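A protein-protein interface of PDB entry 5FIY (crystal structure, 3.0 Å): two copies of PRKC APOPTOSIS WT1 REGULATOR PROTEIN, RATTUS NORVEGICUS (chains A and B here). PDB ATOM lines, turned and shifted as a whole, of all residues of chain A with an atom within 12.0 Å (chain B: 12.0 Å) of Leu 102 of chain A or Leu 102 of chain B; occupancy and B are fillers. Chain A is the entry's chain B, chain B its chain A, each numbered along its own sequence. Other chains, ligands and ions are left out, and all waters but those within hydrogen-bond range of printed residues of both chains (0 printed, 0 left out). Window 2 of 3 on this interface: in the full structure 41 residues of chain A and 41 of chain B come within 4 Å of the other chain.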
ATOM      1  N   LYS A  93     -28.671 -18.264   4.410  1.00  0.00           N
ATOM      2  CA  LYS A  93     -27.980 -17.854   5.622  1.00  0.00           C
ATOM      3  C   LYS A  93     -26.587 -17.347   5.252  1.00  0.00           C
ATOM      4  O   LYS A  93     -26.145 -16.287   5.717  1.00  0.00           O
ATOM      5  CB  LYS A  93     -27.907 -19.039   6.593  1.00  0.00           C
ATOM      6  CG  LYS A  93     -27.389 -18.759   7.991  1.00  0.00           C
ATOM      7  CD  LYS A  93     -27.466 -20.044   8.820  1.00  0.00           C
ATOM      8  CE  LYS A  93     -26.742 -19.927  10.151  1.00  0.00           C
ATOM      9  NZ  LYS A  93     -26.855 -21.182  10.951  1.00  0.00           N
ATOM     10  N   THR A  94     -25.924 -18.089   4.370  1.00  0.00           N
ATOM     11  CA  THR A  94     -24.611 -17.696   3.874  1.00  0.00           C
ATOM     12  C   THR A  94     -24.628 -16.364   3.116  1.00  0.00           C
ATOM     13  O   THR A  94     -23.852 -15.461   3.429  1.00  0.00           O
ATOM     14  CB  THR A  94     -24.025 -18.784   2.960  1.00  0.00           C
ATOM     15  OG1 THR A  94     -23.452 -19.820   3.768  1.00  0.00           O
ATOM     16  CG2 THR A  94     -22.951 -18.209   2.042  1.00  0.00           C
ATOM     17  N   LEU A  95     -25.521 -16.240   2.136  1.00  0.00           N
ATOM     18  CA  LEU A  95     -25.620 -15.026   1.324  1.00  0.00           C
ATOM     19  C   LEU A  95     -25.968 -13.798   2.156  1.00  0.00           C
ATOM     20  O   LEU A  95     -25.412 -12.718   1.962  1.00  0.00           O
ATOM     21  CB  LEU A  95     -26.666 -15.223   0.225  1.00  0.00           C
ATOM     22  CG  LEU A  95     -26.231 -16.144  -0.916  1.00  0.00           C
ATOM     23  CD1 LEU A  95     -27.355 -16.328  -1.922  1.00  0.00           C
ATOM     24  CD2 LEU A  95     -24.975 -15.609  -1.590  1.00  0.00           C
ATOM     25  N   LEU A  96     -26.877 -13.983   3.101  1.00  0.00           N
ATOM     26  CA  LEU A  96     -27.269 -12.933   4.025  1.00  0.00           C
ATOM     27  C   LEU A  96     -26.074 -12.509   4.864  1.00  0.00           C
ATOM     28  O   LEU A  96     -25.861 -11.325   5.107  1.00  0.00           O
ATOM     29  CB  LEU A  96     -28.415 -13.403   4.914  1.00  0.00           C
ATOM     30  CG  LEU A  96     -29.263 -12.310   5.544  1.00  0.00           C
ATOM     31  CD1 LEU A  96     -29.644 -11.269   4.506  1.00  0.00           C
ATOM     32  CD2 LEU A  96     -30.484 -12.972   6.097  1.00  0.00           C
ATOM     33  N   LYS A  97     -25.309 -13.497   5.317  1.00  0.00           N
ATOM     34  CA  LYS A  97     -24.105 -13.248   6.100  1.00  0.00           C
ATOM     35  C   LYS A  97     -23.116 -12.396   5.291  1.00  0.00           C
ATOM     36  O   LYS A  97     -22.542 -11.416   5.792  1.00  0.00           O
ATOM     37  CB  LYS A  97     -23.494 -14.588   6.514  1.00  0.00           C
ATOM     38  CG  LYS A  97     -22.621 -14.572   7.744  1.00  0.00           C
ATOM     39  CD  LYS A  97     -22.477 -15.998   8.266  1.00  0.00           C
ATOM     40  CE  LYS A  97     -21.757 -16.056   9.601  1.00  0.00           C
ATOM     41  NZ  LYS A  97     -21.791 -17.435  10.175  1.00  0.00           N
ATOM     42  N   VAL A  98     -22.950 -12.770   4.025  1.00  0.00           N
ATOM     43  CA  VAL A  98     -22.074 -12.061   3.099  1.00  0.00           C
ATOM     44  C   VAL A  98     -22.495 -10.618   2.910  1.00  0.00           C
ATOM     45  O   VAL A  98     -21.673  -9.708   2.977  1.00  0.00           O
ATOM     46  CB  VAL A  98     -22.057 -12.744   1.732  1.00  0.00           C
ATOM     47  CG1 VAL A  98     -21.252 -11.924   0.733  1.00  0.00           C
ATOM     48  CG2 VAL A  98     -21.474 -14.109   1.874  1.00  0.00           C
ATOM     49  N   VAL A  99     -23.786 -10.412   2.682  1.00  0.00           N
ATOM     50  CA  VAL A  99     -24.313  -9.069   2.503  1.00  0.00           C
ATOM     51  C   VAL A  99     -24.089  -8.268   3.772  1.00  0.00           C
ATOM     52  O   VAL A  99     -23.789  -7.079   3.729  1.00  0.00           O
ATOM     53  CB  VAL A  99     -25.802  -9.091   2.153  1.00  0.00           C
ATOM     54  CG1 VAL A  99     -26.355  -7.685   2.119  1.00  0.00           C
ATOM     55  CG2 VAL A  99     -25.999  -9.742   0.810  1.00  0.00           C
ATOM     56  N   GLY A 100     -24.215  -8.950   4.904  1.00  0.00           N
ATOM     57  CA  GLY A 100     -23.997  -8.349   6.205  1.00  0.00           C
ATOM     58  C   GLY A 100     -22.571  -7.853   6.300  1.00  0.00           C
ATOM     59  O   GLY A 100     -22.315  -6.793   6.870  1.00  0.00           O
ATOM     60  N   GLN A 101     -21.639  -8.616   5.738  1.00  0.00           N
ATOM     61  CA  GLN A 101     -20.243  -8.187   5.739  1.00  0.00           C
ATOM     62  C   GLN A 101     -20.012  -6.996   4.804  1.00  0.00           C
ATOM     63  O   GLN A 101     -19.243  -6.091   5.125  1.00  0.00           O
ATOM     64  CB  GLN A 101     -19.314  -9.339   5.355  1.00  0.00           C
ATOM     65  CG  GLN A 101     -19.221 -10.433   6.403  1.00  0.00           C
ATOM     66  CD  GLN A 101     -17.925 -11.212   6.310  1.00  0.00           C
ATOM     67  OE1 GLN A 101     -17.053 -10.894   5.502  1.00  0.00           O
ATOM     68  NE2 GLN A 101     -17.789 -12.238   7.144  1.00  0.00           N
ATOM     69  N   LEU A 102     -20.674  -6.997   3.653  1.00  0.00           N
ATOM     70  CA  LEU A 102     -20.523  -5.909   2.687  1.00  0.00           C
ATOM     71  C   LEU A 102     -21.234  -4.619   3.110  1.00  0.00           C
ATOM     72  O   LEU A 102     -21.134  -3.599   2.433  1.00  0.00           O
ATOM     73  CB  LEU A 102     -21.053  -6.354   1.325  1.00  0.00           C
ATOM     74  CG  LEU A 102     -20.306  -7.501   0.641  1.00  0.00           C
ATOM     75  CD1 LEU A 102     -20.849  -7.752  -0.761  1.00  0.00           C
ATOM     76  CD2 LEU A 102     -18.807  -7.250   0.616  1.00  0.00           C
ATOM     77  N   THR A 103     -21.949  -4.670   4.230  1.00  0.00           N
ATOM     78  CA  THR A 103     -22.656  -3.505   4.767  1.00  0.00           C
ATOM     79  C   THR A 103     -21.908  -2.857   5.931  1.00  0.00           C
ATOM     80  O   THR A 103     -21.883  -1.629   6.051  1.00  0.00           O
ATOM     81  CB  THR A 103     -24.099  -3.852   5.198  1.00  0.00           C
ATOM     82  OG1 THR A 103     -24.082  -4.993   6.062  1.00  0.00           O
ATOM     83  CG2 THR A 103     -24.945  -4.176   3.976  1.00  0.00           C
ATOM     84  N   ARG A 104     -21.366  -3.685   6.820  1.00  0.00           N
ATOM     85  CA  ARG A 104     -20.573  -3.205   7.950  1.00  0.00           C
ATOM     86  C   ARG A 104     -19.294  -2.495   7.504  1.00  0.00           C
ATOM     87  O   ARG A 104     -19.318  -1.582   6.678  1.00  0.00           O
ATOM     88  CB  ARG A 104     -20.206  -4.367   8.876  1.00  0.00           C
ATOM     89  N   LYS B  93     -32.699 -15.622  -4.916  1.00  0.00           N
ATOM     90  CA  LYS B  93     -32.410 -14.857  -6.128  1.00  0.00           C
ATOM     91  C   LYS B  93     -32.219 -13.370  -5.817  1.00  0.00           C
ATOM     92  O   LYS B  93     -31.308 -12.716  -6.338  1.00  0.00           O
ATOM     93  CB  LYS B  93     -33.526 -15.059  -7.157  1.00  0.00           C
ATOM     94  CG  LYS B  93     -33.214 -14.501  -8.535  1.00  0.00           C
ATOM     95  CD  LYS B  93     -34.322 -14.822  -9.532  1.00  0.00           C
ATOM     96  CE  LYS B  93     -35.539 -13.941  -9.324  1.00  0.00           C
ATOM     97  NZ  LYS B  93     -35.239 -12.517  -9.645  1.00  0.00           N
ATOM     98  N   THR B  94     -33.083 -12.845  -4.953  1.00  0.00           N
ATOM     99  CA  THR B  94     -32.982 -11.460  -4.513  1.00  0.00           C
ATOM    100  C   THR B  94     -31.640 -11.233  -3.827  1.00  0.00           C
ATOM    101  O   THR B  94     -30.939 -10.273  -4.141  1.00  0.00           O
ATOM    102  CB  THR B  94     -34.128 -11.066  -3.556  1.00  0.00           C
ATOM    103  OG1 THR B  94     -35.301 -10.748  -4.317  1.00  0.00           O
ATOM    104  CG2 THR B  94     -33.742  -9.855  -2.719  1.00  0.00           C
ATOM    105  N   LEU B  95     -31.283 -12.115  -2.896  1.00  0.00           N
ATOM    106  CA  LEU B  95     -30.003 -11.979  -2.201  1.00  0.00           C
ATOM    107  C   LEU B  95     -28.810 -12.030  -3.159  1.00  0.00           C
ATOM    108  O   LEU B  95     -27.857 -11.249  -3.018  1.00  0.00           O
ATOM    109  CB  LEU B  95     -29.863 -13.068  -1.138  1.00  0.00           C
ATOM    110  CG  LEU B  95     -30.711 -12.852   0.114  1.00  0.00           C
ATOM    111  CD1 LEU B  95     -30.550 -14.016   1.072  1.00  0.00           C
ATOM    112  CD2 LEU B  95     -30.333 -11.542   0.787  1.00  0.00           C
ATOM    113  N   LEU B  96     -28.880 -12.915  -4.152  1.00  0.00           N
ATOM    114  CA  LEU B  96     -27.823 -12.994  -5.161  1.00  0.00           C
ATOM    115  C   LEU B  96     -27.708 -11.670  -5.912  1.00  0.00           C
ATOM    116  O   LEU B  96     -26.605 -11.156  -6.130  1.00  0.00           O
ATOM    117  CB  LEU B  96     -28.081 -14.144  -6.139  1.00  0.00           C
ATOM    118  CG  LEU B  96     -27.502 -15.500  -5.724  1.00  0.00           C
ATOM    119  CD1 LEU B  96     -28.135 -16.639  -6.511  1.00  0.00           C
ATOM    120  CD2 LEU B  96     -25.990 -15.511  -5.882  1.00  0.00           C
ATOM    121  N   LYS B  97     -28.858 -11.116  -6.287  1.00  0.00           N
ATOM    122  CA  LYS B  97     -28.903  -9.828  -6.971  1.00  0.00           C
ATOM    123  C   LYS B  97     -28.273  -8.719  -6.127  1.00  0.00           C
ATOM    124  O   LYS B  97     -27.503  -7.907  -6.639  1.00  0.00           O
ATOM    125  CB  LYS B  97     -30.346  -9.465  -7.327  1.00  0.00           C
ATOM    126  CG  LYS B  97     -30.479  -8.189  -8.144  1.00  0.00           C
ATOM    127  CD  LYS B  97     -31.883  -8.024  -8.702  1.00  0.00           C
ATOM    128  N   VAL B  98     -28.609  -8.692  -4.840  1.00  0.00           N
ATOM    129  CA  VAL B  98     -28.061  -7.710  -3.908  1.00  0.00           C
ATOM    130  C   VAL B  98     -26.546  -7.824  -3.853  1.00  0.00           C
ATOM    131  O   VAL B  98     -25.833  -6.813  -3.909  1.00  0.00           O
ATOM    132  CB  VAL B  98     -28.637  -7.887  -2.491  1.00  0.00           C
ATOM    133  CG1 VAL B  98     -27.930  -6.961  -1.503  1.00  0.00           C
ATOM    134  CG2 VAL B  98     -30.119  -7.612  -2.502  1.00  0.00           C
ATOM    135  N   VAL B  99     -26.053  -9.056  -3.754  1.00  0.00           N
ATOM    136  CA  VAL B  99     -24.610  -9.266  -3.717  1.00  0.00           C
ATOM    137  C   VAL B  99     -23.993  -8.746  -5.012  1.00  0.00           C
ATOM    138  O   VAL B  99     -22.911  -8.154  -5.004  1.00  0.00           O
ATOM    139  CB  VAL B  99     -24.243 -10.755  -3.525  1.00  0.00           C
ATOM    140  CG1 VAL B  99     -22.743 -10.963  -3.684  1.00  0.00           C
ATOM    141  CG2 VAL B  99     -24.691 -11.244  -2.164  1.00  0.00           C
ATOM    142  N   GLY B 100     -24.703  -8.945  -6.119  1.00  0.00           N
ATOM    143  CA  GLY B 100     -24.243  -8.456  -7.407  1.00  0.00           C
ATOM    144  C   GLY B 100     -24.147  -6.940  -7.489  1.00  0.00           C
ATOM    145  O   GLY B 100     -23.178  -6.406  -8.032  1.00  0.00           O
ATOM    146  N   GLN B 101     -25.139  -6.243  -6.942  1.00  0.00           N
ATOM    147  CA  GLN B 101     -25.127  -4.780  -6.944  1.00  0.00           C
ATOM    148  C   GLN B 101     -24.102  -4.195  -5.989  1.00  0.00           C
ATOM    149  O   GLN B 101     -23.515  -3.154  -6.280  1.00  0.00           O
ATOM    150  CB  GLN B 101     -26.509  -4.199  -6.645  1.00  0.00           C
ATOM    151  CG  GLN B 101     -27.488  -4.372  -7.787  1.00  0.00           C
ATOM    152  CD  GLN B 101     -28.577  -3.319  -7.774  1.00  0.00           C
ATOM    153  OE1 GLN B 101     -28.581  -2.423  -6.929  1.00  0.00           O
ATOM    154  NE2 GLN B 101     -29.479  -3.393  -8.745  1.00  0.00           N
ATOM    155  N   LEU B 102     -23.890  -4.832  -4.843  1.00  0.00           N
ATOM    156  CA  LEU B 102     -22.897  -4.300  -3.920  1.00  0.00           C
ATOM    157  C   LEU B 102     -21.517  -4.492  -4.543  1.00  0.00           C
ATOM    158  O   LEU B 102     -20.919  -3.538  -5.042  1.00  0.00           O
ATOM    159  CB  LEU B 102     -22.979  -4.980  -2.552  1.00  0.00           C
ATOM    160  CG  LEU B 102     -24.247  -4.710  -1.737  1.00  0.00           C
ATOM    161  CD1 LEU B 102     -24.148  -5.328  -0.348  1.00  0.00           C
ATOM    162  CD2 LEU B 102     -24.534  -3.221  -1.646  1.00  0.00           C
ATOM    163  N   THR B 103     -21.014  -5.720  -4.526  1.00  0.00           N
ATOM    164  CA  THR B 103     -19.731  -6.008  -5.150  1.00  0.00           C
ATOM    165  C   THR B 103     -19.932  -6.674  -6.510  1.00  0.00           C
ATOM    166  O   THR B 103     -20.260  -6.014  -7.497  1.00  0.00           O
ATOM    167  CB  THR B 103     -18.855  -6.902  -4.262  1.00  0.00           C
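Leu 95 of chain A touches Leu 96 of chain B, and with the chains exchanged Leu 96 of chain A touches Leu 95 of chain B.
Val 99 of chain A touches its own counterpart, Val 99 of chain B.
Leu 102 of chain B touches its own counterpart, Leu 102 of chain A.
11 positions are printed for both chains.
Of the 4 pairs that touch across the chains among the printed residues, 4 have their exchanged pair printed and touching as well.
Of the 12 printed residues of chain A, 4 touch a printed residue of chain B.
Hydrophobic or aromatic side chains of chain A within 4 Å of the printed part of chain B: Leu 95, Leu 96, Val 99 and Leu 102.
Hydrophobic or aromatic side chains of chain B within 4 Å of the printed part of chain A: Leu 95, Leu 96, Val 99 and Leu 102.
O of Val 99 of chain A lies close to OG1 of Thr 103 of chain A (3.1 Å).
Leu 102 of chain A touches just one residue of chain B: Leu 102 (3.7 Å).
No residue of chain B comes within 4 Å of Gly 100 of chain A.
No residue of chain B comes within 4 Å of Gln 101 of chain A.
No residue of chain B comes within 4 Å of Thr 103 of chain A.
No residue of chain B comes within 4 Å of Arg 104 of chain A.
Of chain A, only Val 99 (3.6 Å) comes within 4 Å of Val 99 of chain B.
No residue of chain A comes within 4 Å of Gly 100 of chain B.
No residue of chain A comes within 4 Å of Thr 103 of chain B.
Of the printed residues of chain B, Leu 95 of chain A touches Leu 96 (3.9 Å).
Of the printed residues of chain A, Leu 95 of chain B touches Leu 96 (3.8 Å).
Printed residues of chain A within 4 Å of Leu 96 of chain B: Leu 95 (3.9 Å).
Of the printed residues of chain B, Leu 96 of chain A touches Leu 95 (3.8 Å).
Val 98 of chain B touches none of the printed residues of chain A.
Lys 93 of chain B touches none of the printed residues of chain A.
The nearest residue of chain B that does not touch Leu 102 of chain A is Thr 103 of chain B (4.1 Å).
The nearest residue of chain A that does not touch Leu 102 of chain B is Val 99 of chain A (4.1 Å).
Among the printed residues, pairs that only touch across the chains: Leu 95 of chain A with Leu 96 of chain B (3.9 Å), Leu 96 of chain A with Leu 95 of chain B (3.8 Å), Val 99 of chain A with Val 99 of chain B (3.6 Å) and Leu 102 of chain A with Leu 102 of chain B (3.7 Å).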
